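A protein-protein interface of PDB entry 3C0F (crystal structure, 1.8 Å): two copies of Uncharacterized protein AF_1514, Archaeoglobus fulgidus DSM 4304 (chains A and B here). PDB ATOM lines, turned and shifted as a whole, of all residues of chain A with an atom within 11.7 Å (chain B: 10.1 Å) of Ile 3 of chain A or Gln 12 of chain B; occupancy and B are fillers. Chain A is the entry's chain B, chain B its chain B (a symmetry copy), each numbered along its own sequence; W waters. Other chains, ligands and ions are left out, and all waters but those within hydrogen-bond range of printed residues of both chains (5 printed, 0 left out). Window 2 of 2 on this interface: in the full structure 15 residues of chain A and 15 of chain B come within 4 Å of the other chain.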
ATOM      1  N   ILE A   3      -7.363  -1.972  -4.377  1.00  0.00           N
ATOM      2  CA  ILE A   3      -6.056  -2.355  -3.856  1.00  0.00           C
ATOM      3  C   ILE A   3      -5.650  -1.468  -2.683  1.00  0.00           C
ATOM      4  O   ILE A   3      -5.653  -0.231  -2.791  1.00  0.00           O
ATOM      5  CB  ILE A   3      -5.007  -2.296  -4.956  1.00  0.00           C
ATOM      6  N   MET A   4      -5.334  -2.100  -1.560  1.00  0.00           N
ATOM      7  CA  MET A   4      -4.932  -1.415  -0.334  1.00  0.00           C
ATOM      8  C   MET A   4      -3.731  -2.134   0.282  1.00  0.00           C
ATOM      9  O   MET A   4      -3.367  -3.224  -0.161  1.00  0.00           O
ATOM     10  CB  MET A   4      -6.099  -1.377   0.664  1.00  0.00           C
ATOM     11  CG  MET A   4      -6.533  -2.749   1.199  1.00  0.00           C
ATOM     12  SD  MET A   4      -8.137  -2.755   2.040  1.00  0.00           S
ATOM     13  CE  MET A   4      -9.254  -2.583   0.657  1.00  0.00           C
ATOM     14  N   ASP A   5      -3.128  -1.527   1.303  1.00  0.00           N
ATOM     15  CA  ASP A   5      -2.084  -2.197   2.082  1.00  0.00           C
ATOM     16  C   ASP A   5      -2.647  -3.468   2.719  1.00  0.00           C
ATOM     17  O   ASP A   5      -3.807  -3.497   3.144  1.00  0.00           O
ATOM     18  CB  ASP A   5      -1.520  -1.268   3.159  1.00  0.00           C
ATOM     19  CG  ASP A   5      -0.665  -0.139   2.584  1.00  0.00           C
ATOM     20  OD1 ASP A   5      -0.296  -0.188   1.390  1.00  0.00           O
ATOM     21  OD2 ASP A   5      -0.359   0.801   3.344  1.00  0.00           O
ATOM     22  N   GLU A   6      -1.828  -4.515   2.763  1.00  0.00           N
ATOM     23  CA  GLU A   6      -2.274  -5.827   3.235  1.00  0.00           C
ATOM     24  C   GLU A   6      -1.306  -6.442   4.238  1.00  0.00           C
ATOM     25  O   GLU A   6      -0.089  -6.321   4.101  1.00  0.00           O
ATOM     26  CB  GLU A   6      -2.455  -6.792   2.055  1.00  0.00           C
ATOM     27  CG  GLU A   6      -3.570  -6.420   1.091  1.00  0.00           C
ATOM     28  CD  GLU A   6      -3.719  -7.406  -0.059  1.00  0.00           C
ATOM     29  OE1 GLU A   6      -3.202  -8.540   0.037  1.00  0.00           O
ATOM     30  OE2 GLU A   6      -4.364  -7.042  -1.063  1.00  0.00           O
ATOM     31  N   ILE A   7      -1.864  -7.106   5.243  1.00  0.00           N
ATOM     32  CA  ILE A   7      -1.077  -7.875   6.204  1.00  0.00           C
ATOM     33  C   ILE A   7      -1.713  -9.259   6.308  1.00  0.00           C
ATOM     34  O   ILE A   7      -2.904  -9.381   6.610  1.00  0.00           O
ATOM     35  CB  ILE A   7      -1.003  -7.176   7.593  1.00  0.00           C
ATOM     36  CG1 ILE A   7      -0.312  -5.807   7.474  1.00  0.00           C
ATOM     37  CG2 ILE A   7      -0.272  -8.061   8.616  1.00  0.00           C
ATOM     38  CD1 ILE A   7      -0.398  -4.919   8.717  1.00  0.00           C
ATOM     39  N   TYR A  31      -1.038   1.462  13.699  1.00  0.00           N
ATOM     40  CA  TYR A  31      -1.082   2.405  12.575  1.00  0.00           C
ATOM     41  C   TYR A  31      -2.073   3.549  12.764  1.00  0.00           C
ATOM     42  O   TYR A  31      -2.031   4.546  12.040  1.00  0.00           O
ATOM     43  CB  TYR A  31      -1.326   1.645  11.265  1.00  0.00           C
ATOM     44  CG  TYR A  31      -0.410   0.448  11.152  1.00  0.00           C
ATOM     45  CD1 TYR A  31       0.973   0.615  11.045  1.00  0.00           C
ATOM     46  CD2 TYR A  31      -0.917  -0.850  11.207  1.00  0.00           C
ATOM     47  CE1 TYR A  31       1.827  -0.479  10.968  1.00  0.00           C
ATOM     48  CE2 TYR A  31      -0.070  -1.957  11.127  1.00  0.00           C
ATOM     49  CZ  TYR A  31       1.298  -1.763  11.009  1.00  0.00           C
ATOM     50  OH  TYR A  31       2.141  -2.846  10.934  1.00  0.00           O
ATOM     51  N   LYS A  57     -17.690 -10.981  -3.771  1.00  0.00           N
ATOM     52  CA  LYS A  57     -17.065 -10.488  -2.527  1.00  0.00           C
ATOM     53  C   LYS A  57     -17.722  -9.214  -1.962  1.00  0.00           C
ATOM     54  O   LYS A  57     -17.050  -8.191  -1.798  1.00  0.00           O
ATOM     55  CB  LYS A  57     -15.554 -10.273  -2.720  1.00  0.00           C
ATOM     56  CG  LYS A  57     -14.784 -11.506  -3.185  1.00  0.00           C
ATOM     57  CD  LYS A  57     -13.321 -11.173  -3.455  1.00  0.00           C
ATOM     58  N   GLU A  60     -16.141  -7.086   0.824  1.00  0.00           N
ATOM     59  CA  GLU A  60     -14.993  -6.286   0.407  1.00  0.00           C
ATOM     60  C   GLU A  60     -15.452  -5.007  -0.290  1.00  0.00           C
ATOM     61  O   GLU A  60     -14.934  -3.923  -0.011  1.00  0.00           O
ATOM     62  CB  GLU A  60     -14.063  -7.104  -0.492  1.00  0.00           C
ATOM     63  CG  GLU A  60     -12.799  -6.367  -0.913  1.00  0.00           C
ATOM     64  CD  GLU A  60     -11.718  -7.296  -1.436  1.00  0.00           C
ATOM     65  OE1 GLU A  60     -12.049  -8.298  -2.104  1.00  0.00           O
ATOM     66  OE2 GLU A  60     -10.531  -7.017  -1.179  1.00  0.00           O
ATOM     67  N   VAL A  61     -16.426  -5.142  -1.189  1.00  0.00           N
ATOM     68  CA  VAL A  61     -17.025  -3.996  -1.875  1.00  0.00           C
ATOM     69  C   VAL A  61     -17.588  -3.000  -0.856  1.00  0.00           C
ATOM     70  O   VAL A  61     -17.334  -1.797  -0.955  1.00  0.00           O
ATOM     71  CB  VAL A  61     -18.123  -4.436  -2.884  1.00  0.00           C
ATOM     72  CG1 VAL A  61     -18.737  -3.228  -3.586  1.00  0.00           C
ATOM     73  CG2 VAL A  61     -17.549  -5.411  -3.910  1.00  0.00           C
ATOM     74  N   ALA A  63     -16.712  -2.573   2.315  1.00  0.00           N
ATOM     75  CA  ALA A  63     -15.603  -1.948   3.027  1.00  0.00           C
ATOM     76  C   ALA A  63     -14.907  -0.882   2.179  1.00  0.00           C
ATOM     77  O   ALA A  63     -14.647   0.223   2.654  1.00  0.00           O
ATOM     78  CB  ALA A  63     -14.615  -3.006   3.484  1.00  0.00           C
ATOM     79  N   CYS A  64     -14.632  -1.215   0.919  1.00  0.00           N
ATOM     80  CA  CYS A  64     -13.939  -0.303   0.007  1.00  0.00           C
ATOM     81  C   CYS A  64     -14.739   0.968  -0.265  1.00  0.00           C
ATOM     82  O   CYS A  64     -14.164   2.054  -0.398  1.00  0.00           O
ATOM     83  CB  CYS A  64     -13.583  -1.018  -1.294  1.00  0.00           C
ATOM     84  SG  CYS A  64     -12.293  -2.269  -1.077  1.00  0.00           S
ATOM     85  N   ASN A  65     -16.062   0.826  -0.325  1.00  0.00           N
ATOM     86  CA  ASN A  65     -16.968   1.966  -0.451  1.00  0.00           C
ATOM     87  C   ASN A  65     -17.009   2.846   0.806  1.00  0.00           C
ATOM     88  O   ASN A  65     -17.474   3.987   0.750  1.00  0.00           O
ATOM     89  CB  ASN A  65     -18.378   1.496  -0.830  1.00  0.00           C
ATOM     90  CG  ASN A  65     -18.459   0.957  -2.256  1.00  0.00           C
ATOM     91  OD1 ASN A  65     -17.532   1.119  -3.053  1.00  0.00           O
ATOM     92  ND2 ASN A  65     -19.575   0.315  -2.581  1.00  0.00           N
ATOM     93  N   GLY A  67     -14.113   3.476   2.494  1.00  0.00           N
ATOM     94  CA  GLY A  67     -12.741   3.960   2.647  1.00  0.00           C
ATOM     95  C   GLY A  67     -11.779   3.025   3.359  1.00  0.00           C
ATOM     96  O   GLY A  67     -10.832   3.482   4.010  1.00  0.00           O
ATOM     97  N   ALA A  68     -12.006   1.718   3.234  1.00  0.00           N
ATOM     98  CA  ALA A  68     -11.066   0.731   3.764  1.00  0.00           C
ATOM     99  C   ALA A  68      -9.680   0.974   3.169  1.00  0.00           C
ATOM    100  O   ALA A  68      -9.548   1.205   1.963  1.00  0.00           O
ATOM    101  CB  ALA A  68     -11.536  -0.681   3.462  1.00  0.00           C
ATOM    102  N   ASN A  69      -8.659   0.940   4.021  1.00  0.00           N
ATOM    103  CA  ASN A  69      -7.280   1.165   3.582  1.00  0.00           C
ATOM    104  C   ASN A  69      -6.268   0.154   4.128  1.00  0.00           C
ATOM    105  O   ASN A  69      -5.067   0.270   3.877  1.00  0.00           O
ATOM    106  CB  ASN A  69      -6.832   2.606   3.880  1.00  0.00           C
ATOM    107  CG  ASN A  69      -6.993   2.991   5.350  1.00  0.00           C
ATOM    108  OD1 ASN A  69      -7.204   2.141   6.216  1.00  0.00           O
ATOM    109  ND2 ASN A  69      -6.893   4.285   5.630  1.00  0.00           N
ATOM    110  N   LEU A  70      -6.760  -0.833   4.876  1.00  0.00           N
ATOM    111  CA  LEU A  70      -5.909  -1.910   5.384  1.00  0.00           C
ATOM    112  C   LEU A  70      -6.678  -3.222   5.512  1.00  0.00           C
ATOM    113  O   LEU A  70      -7.690  -3.297   6.214  1.00  0.00           O
ATOM    114  CB  LEU A  70      -5.272  -1.531   6.728  1.00  0.00           C
ATOM    115  CG  LEU A  70      -4.296  -2.525   7.375  1.00  0.00           C
ATOM    116  CD1 LEU A  70      -3.064  -2.794   6.506  1.00  0.00           C
ATOM    117  CD2 LEU A  70      -3.878  -2.025   8.748  1.00  0.00           C
ATOM    118  N   MLY A  71      -6.184  -4.242   4.818  1.00  0.00           N
ATOM    119  CA  MLY A  71      -6.733  -5.589   4.896  1.00  0.00           C
ATOM    120  CB  MLY A  71      -6.832  -6.142   3.478  1.00  0.00           C
ATOM    121  CG  MLY A  71      -7.290  -7.595   3.421  1.00  0.00           C
ATOM    122  CD  MLY A  71      -6.993  -8.175   2.042  1.00  0.00           C
ATOM    123  CE  MLY A  71      -7.698  -9.513   1.849  1.00  0.00           C
ATOM    124  NZ  MLY A  71      -7.417 -10.091   0.520  1.00  0.00           N
ATOM    125  CH1 MLY A  71      -8.117  -9.352  -0.540  1.00  0.00           C
ATOM    126  CH2 MLY A  71      -7.895 -11.479   0.498  1.00  0.00           C
ATOM    127  C   MLY A  71      -5.828  -6.445   5.733  1.00  0.00           C
ATOM    128  O   MLY A  71      -4.643  -6.577   5.433  1.00  0.00           O
ATOM    129  N   ILE A  72      -6.375  -7.029   6.796  1.00  0.00           N
ATOM    130  CA  ILE A  72      -5.603  -7.944   7.639  1.00  0.00           C
ATOM    131  C   ILE A  72      -6.243  -9.328   7.628  1.00  0.00           C
ATOM    132  O   ILE A  72      -7.406  -9.489   8.016  1.00  0.00           O
ATOM    133  CB  ILE A  72      -5.447  -7.437   9.101  1.00  0.00           C
ATOM    134  CG1 ILE A  72      -4.744  -6.070   9.133  1.00  0.00           C
ATOM    135  CG2 ILE A  72      -4.683  -8.472   9.949  1.00  0.00           C
ATOM    136  CD1 ILE A  72      -4.768  -5.385  10.494  1.00  0.00           C
ATOM    137  N   PHE A  79     -10.087  -9.338   7.502  1.00  0.00           N
ATOM    138  CA  PHE A  79     -10.653  -8.173   8.171  1.00  0.00           C
ATOM    139  C   PHE A  79     -10.318  -6.922   7.374  1.00  0.00           C
ATOM    140  O   PHE A  79      -9.164  -6.698   7.021  1.00  0.00           O
ATOM    141  CB  PHE A  79     -10.082  -8.042   9.586  1.00  0.00           C
ATOM    142  CG  PHE A  79     -10.396  -9.208  10.478  1.00  0.00           C
ATOM    143  CD1 PHE A  79     -11.550  -9.213  11.248  1.00  0.00           C
ATOM    144  CD2 PHE A  79      -9.532 -10.302  10.550  1.00  0.00           C
ATOM    145  CE1 PHE A  79     -11.851 -10.295  12.080  1.00  0.00           C
ATOM    146  CE2 PHE A  79      -9.825 -11.390  11.378  1.00  0.00           C
ATOM    147  CZ  PHE A  79     -10.987 -11.387  12.138  1.00  0.00           C
ATOM    148  N   TYR A  80     -11.333  -6.110   7.100  1.00  0.00           N
ATOM    149  CA  TYR A  80     -11.137  -4.877   6.347  1.00  0.00           C
ATOM    150  C   TYR A  80     -11.337  -3.668   7.256  1.00  0.00           C
ATOM    151  O   TYR A  80     -12.428  -3.462   7.802  1.00  0.00           O
ATOM    152  CB  TYR A  80     -12.074  -4.838   5.136  1.00  0.00           C
ATOM    153  CG  TYR A  80     -11.784  -5.924   4.123  1.00  0.00           C
ATOM    154  CD1 TYR A  80     -10.931  -5.686   3.044  1.00  0.00           C
ATOM    155  CD2 TYR A  80     -12.344  -7.197   4.254  1.00  0.00           C
ATOM    156  CE1 TYR A  80     -10.651  -6.689   2.115  1.00  0.00           C
ATOM    157  CE2 TYR A  80     -12.070  -8.205   3.333  1.00  0.00           C
ATOM    158  CZ  TYR A  80     -11.222  -7.942   2.270  1.00  0.00           C
ATOM    159  OH  TYR A  80     -10.950  -8.936   1.358  1.00  0.00           O
ATOM    160  N   PHE A  81     -10.268  -2.885   7.414  1.00  0.00           N
ATOM    161  CA  PHE A  81     -10.247  -1.716   8.292  1.00  0.00           C
ATOM    162  C   PHE A  81     -10.151  -0.405   7.518  1.00  0.00           C
ATOM    163  O   PHE A  81      -9.487  -0.338   6.479  1.00  0.00           O
ATOM    164  CB  PHE A  81      -9.011  -1.756   9.203  1.00  0.00           C
ATOM    165  CG  PHE A  81      -9.041  -2.820  10.262  1.00  0.00           C
ATOM    166  CD1 PHE A  81      -9.583  -2.557  11.519  1.00  0.00           C
ATOM    167  CD2 PHE A  81      -8.475  -4.070  10.026  1.00  0.00           C
ATOM    168  CE1 PHE A  81      -9.588  -3.539  12.516  1.00  0.00           C
ATOM    169  CE2 PHE A  81      -8.476  -5.058  11.014  1.00  0.00           C
ATOM    170  CZ  PHE A  81      -9.030  -4.788  12.265  1.00  0.00           C
ATOM    171  N   ILE A  83      -8.278   2.667   8.684  1.00  0.00           N
ATOM    172  CA  ILE A  83      -7.369   3.201   9.691  1.00  0.00           C
ATOM    173  C   ILE A  83      -7.468   4.722   9.663  1.00  0.00           C
ATOM    174  O   ILE A  83      -7.151   5.357   8.653  1.00  0.00           O
ATOM    175  CB  ILE A  83      -5.896   2.750   9.468  1.00  0.00           C
ATOM    176  CG1 ILE A  83      -5.777   1.216   9.378  1.00  0.00           C
ATOM    177  CG2 ILE A  83      -4.968   3.342  10.547  1.00  0.00           C
ATOM    178  CD1 ILE A  83      -6.180   0.441  10.644  1.00  0.00           C
ATOM    179  N   VAL B   9       3.613  -8.712   5.084  1.00  0.00           N
ATOM    180  CA  VAL B   9       3.127  -7.354   4.861  1.00  0.00           C
ATOM    181  C   VAL B   9       3.404  -6.927   3.418  1.00  0.00           C
ATOM    182  O   VAL B   9       4.536  -7.025   2.940  1.00  0.00           O
ATOM    183  CB  VAL B   9       3.774  -6.351   5.849  1.00  0.00           C
ATOM    184  CG1 VAL B   9       3.194  -4.955   5.660  1.00  0.00           C
ATOM    185  CG2 VAL B   9       3.585  -6.817   7.295  1.00  0.00           C
ATOM    186  N   ASN B  10       2.354  -6.471   2.739  1.00  0.00           N
ATOM    187  CA  ASN B  10       2.447  -5.954   1.376  1.00  0.00           C
ATOM    188  C   ASN B  10       1.980  -4.504   1.330  1.00  0.00           C
ATOM    189  O   ASN B  10       0.780  -4.222   1.389  1.00  0.00           O
ATOM    190  CB  ASN B  10       1.629  -6.821   0.414  1.00  0.00           C
ATOM    191  CG  ASN B  10       2.153  -8.242   0.321  1.00  0.00           C
ATOM    192  OD1 ASN B  10       3.320  -8.463   0.005  1.00  0.00           O
ATOM    193  ND2 ASN B  10       1.289  -9.213   0.588  1.00  0.00           N
ATOM    194  N   LEU B  11       2.942  -3.589   1.250  1.00  0.00           N
ATOM    195  CA  LEU B  11       2.659  -2.158   1.237  1.00  0.00           C
ATOM    196  C   LEU B  11       2.738  -1.608  -0.178  1.00  0.00           C
ATOM    197  O   LEU B  11       3.592  -2.021  -0.969  1.00  0.00           O
ATOM    198  CB  LEU B  11       3.626  -1.400   2.157  1.00  0.00           C
ATOM    199  CG  LEU B  11       3.723  -1.804   3.636  1.00  0.00           C
ATOM    200  CD1 LEU B  11       4.866  -1.059   4.312  1.00  0.00           C
ATOM    201  CD2 LEU B  11       2.408  -1.567   4.382  1.00  0.00           C
ATOM    202  N   GLN B  12       1.838  -0.678  -0.487  1.00  0.00           N
ATOM    203  CA  GLN B  12       1.799  -0.034  -1.800  1.00  0.00           C
ATOM    204  C   GLN B  12       3.061   0.783  -2.085  1.00  0.00           C
ATOM    205  O   GLN B  12       3.538   0.826  -3.221  1.00  0.00           O
ATOM    206  CB  GLN B  12       0.555   0.848  -1.929  1.00  0.00           C
ATOM    207  CG  GLN B  12      -0.733   0.073  -2.147  1.00  0.00           C
ATOM    208  CD  GLN B  12      -1.961   0.963  -2.083  1.00  0.00           C
ATOM    209  OE1 GLN B  12      -2.346   1.430  -1.011  1.00  0.00           O
ATOM    210  NE2 GLN B  12      -2.582   1.199  -3.233  1.00  0.00           N
ATOM    211  N   LYS B  13       3.601   1.417  -1.048  1.00  0.00           N
ATOM    212  CA  LYS B  13       4.811   2.218  -1.187  1.00  0.00           C
ATOM    213  C   LYS B  13       6.069   1.349  -1.183  1.00  0.00           C
ATOM    214  O   LYS B  13       6.059   0.219  -0.682  1.00  0.00           O
ATOM    215  CB  LYS B  13       4.890   3.286  -0.088  1.00  0.00           C
ATOM    216  CG  LYS B  13       5.181   2.760   1.314  1.00  0.00           C
ATOM    217  CD  LYS B  13       5.426   3.909   2.276  1.00  0.00           C
ATOM    218  CE  LYS B  13       5.720   3.413   3.676  1.00  0.00           C
ATOM    219  NZ  LYS B  13       5.923   4.552   4.615  1.00  0.00           N
ATOM    220  N   GLU B  14       7.144   1.884  -1.754  1.00  0.00           N
ATOM    221  CA  GLU B  14       8.448   1.235  -1.706  1.00  0.00           C
ATOM    222  C   GLU B  14       9.108   1.508  -0.359  1.00  0.00           C
ATOM    223  O   GLU B  14       8.990   2.610   0.187  1.00  0.00           O
ATOM    224  CB  GLU B  14       9.343   1.720  -2.848  1.00  0.00           C
ATOM    225  CG  GLU B  14       8.887   1.290  -4.244  1.00  0.00           C
ATOM    226  CD  GLU B  14       9.220  -0.163  -4.578  1.00  0.00           C
ATOM    227  OE1 GLU B  14       9.849  -0.860  -3.751  1.00  0.00           O
ATOM    228  OE2 GLU B  14       8.851  -0.609  -5.686  1.00  0.00           O
ATOM    229  N   VAL B  15       9.785   0.494   0.177  1.00  0.00           N
ATOM    230  CA  VAL B  15      10.455   0.606   1.470  1.00  0.00           C
ATOM    231  C   VAL B  15      11.950   0.316   1.377  1.00  0.00           C
ATOM    232  O   VAL B  15      12.386  -0.530   0.588  1.00  0.00           O
ATOM    233  CB  VAL B  15       9.812  -0.306   2.561  1.00  0.00           C
ATOM    234  CG1 VAL B  15       8.409   0.178   2.914  1.00  0.00           C
ATOM    235  CG2 VAL B  15       9.799  -1.778   2.130  1.00  0.00           C
ATOM    236  N   TYR B  23       9.218  -1.429  10.517  1.00  0.00           N
ATOM    237  CA  TYR B  23       7.875  -2.018  10.369  1.00  0.00           C
ATOM    238  C   TYR B  23       7.781  -3.410  11.006  1.00  0.00           C
ATOM    239  O   TYR B  23       6.831  -3.705  11.745  1.00  0.00           O
ATOM    240  CB  TYR B  23       7.482  -2.120   8.887  1.00  0.00           C
ATOM    241  CG  TYR B  23       6.772  -0.916   8.305  1.00  0.00           C
ATOM    242  CD1 TYR B  23       7.418  -0.073   7.397  1.00  0.00           C
ATOM    243  CD2 TYR B  23       5.446  -0.634   8.632  1.00  0.00           C
ATOM    244  CE1 TYR B  23       6.768   1.030   6.844  1.00  0.00           C
ATOM    245  CE2 TYR B  23       4.785   0.464   8.085  1.00  0.00           C
ATOM    246  CZ  TYR B  23       5.453   1.291   7.194  1.00  0.00           C
ATOM    247  OH  TYR B  23       4.808   2.377   6.653  1.00  0.00           O
ATOM    248  N   MLY B  43      14.896  -8.990  -3.557  1.00  0.00           N
ATOM    249  CA  MLY B  43      15.165  -8.223  -4.775  1.00  0.00           C
ATOM    250  CB  MLY B  43      14.635  -6.806  -4.596  1.00  0.00           C
ATOM    251  CG  MLY B  43      14.363  -6.099  -5.914  1.00  0.00           C
ATOM    252  CD  MLY B  43      13.344  -4.993  -5.670  1.00  0.00           C
ATOM    253  CE  MLY B  43      13.105  -4.166  -6.928  1.00  0.00           C
ATOM    254  NZ  MLY B  43      12.982  -2.737  -6.595  1.00  0.00           N
ATOM    255  CH1 MLY B  43      11.742  -2.482  -5.846  1.00  0.00           C
ATOM    256  CH2 MLY B  43      12.955  -1.958  -7.840  1.00  0.00           C
ATOM    257  C   MLY B  43      16.631  -8.186  -5.131  1.00  0.00           C
ATOM    258  O   MLY B  43      16.988  -8.278  -6.308  1.00  0.00           O
ATOM    259  N   VAL B  74       8.221  -7.887   4.846  1.00  0.00           N
ATOM    260  CA  VAL B  74       7.753  -6.544   4.507  1.00  0.00           C
ATOM    261  C   VAL B  74       8.217  -6.269   3.081  1.00  0.00           C
ATOM    262  O   VAL B  74       9.420  -6.102   2.827  1.00  0.00           O
ATOM    263  CB  VAL B  74       8.287  -5.468   5.496  1.00  0.00           C
ATOM    264  CG1 VAL B  74       7.734  -4.087   5.148  1.00  0.00           C
ATOM    265  CG2 VAL B  74       7.944  -5.839   6.941  1.00  0.00           C
ATOM    266  N   ASN B  75       7.257  -6.237   2.157  1.00  0.00           N
ATOM    267  CA  ASN B  75       7.542  -6.236   0.718  1.00  0.00           C
ATOM    268  C   ASN B  75       8.631  -7.264   0.357  1.00  0.00           C
ATOM    269  O   ASN B  75       8.447  -8.458   0.609  1.00  0.00           O
ATOM    270  CB  ASN B  75       7.848  -4.815   0.214  1.00  0.00           C
ATOM    271  CG  ASN B  75       6.634  -3.893   0.288  1.00  0.00           C
ATOM    272  OD1 ASN B  75       5.560  -4.291   0.752  1.00  0.00           O
ATOM    273  ND2 ASN B  75       6.801  -2.651  -0.167  1.00  0.00           N
ATOM    274  N   GLN B  76       9.763  -6.809  -0.185  1.00  0.00           N
ATOM    275  CA  GLN B  76      10.831  -7.715  -0.631  1.00  0.00           C
ATOM    276  C   GLN B  76      11.713  -8.287   0.489  1.00  0.00           C
ATOM    277  O   GLN B  76      12.560  -9.148   0.236  1.00  0.00           O
ATOM    278  CB  GLN B  76      11.715  -7.040  -1.693  1.00  0.00           C
ATOM    279  CG  GLN B  76      12.604  -5.908  -1.175  1.00  0.00           C
ATOM    280  CD  GLN B  76      11.978  -4.532  -1.329  1.00  0.00           C
ATOM    281  OE1 GLN B  76      10.777  -4.351  -1.125  1.00  0.00           O
ATOM    282  NE2 GLN B  76      12.799  -3.550  -1.694  1.00  0.00           N
HETATM  283  O   HOH W   1       1.880   1.867   1.597  1.00  0.00           O
HETATM  284  O   HOH W   2      -0.783  -4.114  -1.008  1.00  0.00           O
HETATM  285  O   HOH W   3       0.070  -9.498   2.665  1.00  0.00           O
HETATM  286  O   HOH W   4       4.639  -1.936  11.881  1.00  0.00           O
HETATM  287  O   HOH W   5      -3.976   1.252   1.742  1.00  0.00           O
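N of MLY 71 of chain A lies within hydrogen-bond range of the backbone carbonyl oxygen of Asp 5 of chain A (3.0 Å).
N of MLY 71 of chain A sits at hydrogen-bond distance from SD of Met 4 of chain A (3.7 Å).
N of Leu 11 of chain B lies within hydrogen-bond range of OD1 of Asn 75 of chain B (2.8 Å).
The side-chain sulfur of Met 4 of chain A sits at hydrogen-bond distance from the backbone NH of Leu 70 of chain A (3.7 Å).
O of Val 9 of chain B is in hydrogen-bond range of N of Asn 75 of chain B.
Met 4 of chain A touches Gln 12 of chain B.
Asp 5 of chain A touches Asn 10 of chain B.
CA of Leu 11 of chain B touches OD1 of Asp 5 of chain A, 3.6 Å away.
CA of Val 9 of chain B touches O of Glu 6 of chain A (3.5 Å).
The backbone carbonyl oxygen (O) of Glu 6 of chain A is in hydrogen-bond range of the backbone NH (N) of Asn 10 of chain B, 2.8 Å away.
The backbone NH (N) of Gln 12 of chain B lies within hydrogen-bond range of the side-chain carboxylate (OD1) of Asp 5 of chain A (2.9 Å).
The side-chain amide nitrogen (NE2) of Gln 12 of chain B is in hydrogen-bond range of the backbone carbonyl oxygen (O) of Ile 3 of chain A, 3.4 Å away.
No position is printed for both chains.
Along chain A the printed residues that touch a printed residue of chain B span positions 3 to 6.
Printed residues of chain B that touch a printed residue of chain A: Val 9, Asn 10, Leu 11 and Gln 12.
Hydrophobic or aromatic side chains of chain B within 4 Å of the printed part of chain A: Val 9 and Leu 11.
Among the printed residues, 7 pairs touch across the chains.
Of the printed residues of chain B, Asp 5 of chain A touches Asn 10, Leu 11 and Gln 12.
Of the printed residues of chain B, Glu 6 of chain A touches Val 9 (3.5 Å) and Asn 10 (2.8 Å).
Printed residues of chain A within 4 Å of Val 9 of chain B: Glu 6.
Leu 11 of chain B touches just one residue of chain A: Asp 5 (3.6 Å).
Of chain A, only Ile 3, Met 4 and Asp 5 come within 4 Å of Gln 12 of chain B.
Glu 14 of chain B touches none of the printed residues of chain A.
The nearest residue of chain B that does not touch Ile 3 of chain A is Asn 10 of chain B (8.1 Å).
Water W3 lies within hydrogen-bond range of the side-chain amide nitrogen (ND2) of Asn 10 of chain B (2.4 Å) and the backbone carbonyl oxygen (O) of Glu 6 of chain A (3.5 Å).
Water W5 lies within hydrogen-bond range of the backbone carbonyl oxygen (O) of Asn 69 of chain A, the backbone NH (N) of Asp 5 of chain A and the side-chain amide oxygen (OE1) of Gln 12 of chain B.
Water W4 lies within hydrogen-bond range of O of Tyr 23 of chain B and OH of Tyr 31 of chain A.
Water W2 bridges O of Met 4 of chain A (2.9 Å) and O of Asn 10 of chain B (2.9 Å).
Water W1 lies within hydrogen-bond range of the side-chain carboxylate of Asp 5 of chain A (3.0 Å), the backbone NH of Lys 13 of chain B (3.2 Å) and the backbone NH of Gln 12 of chain B (3.3 Å).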
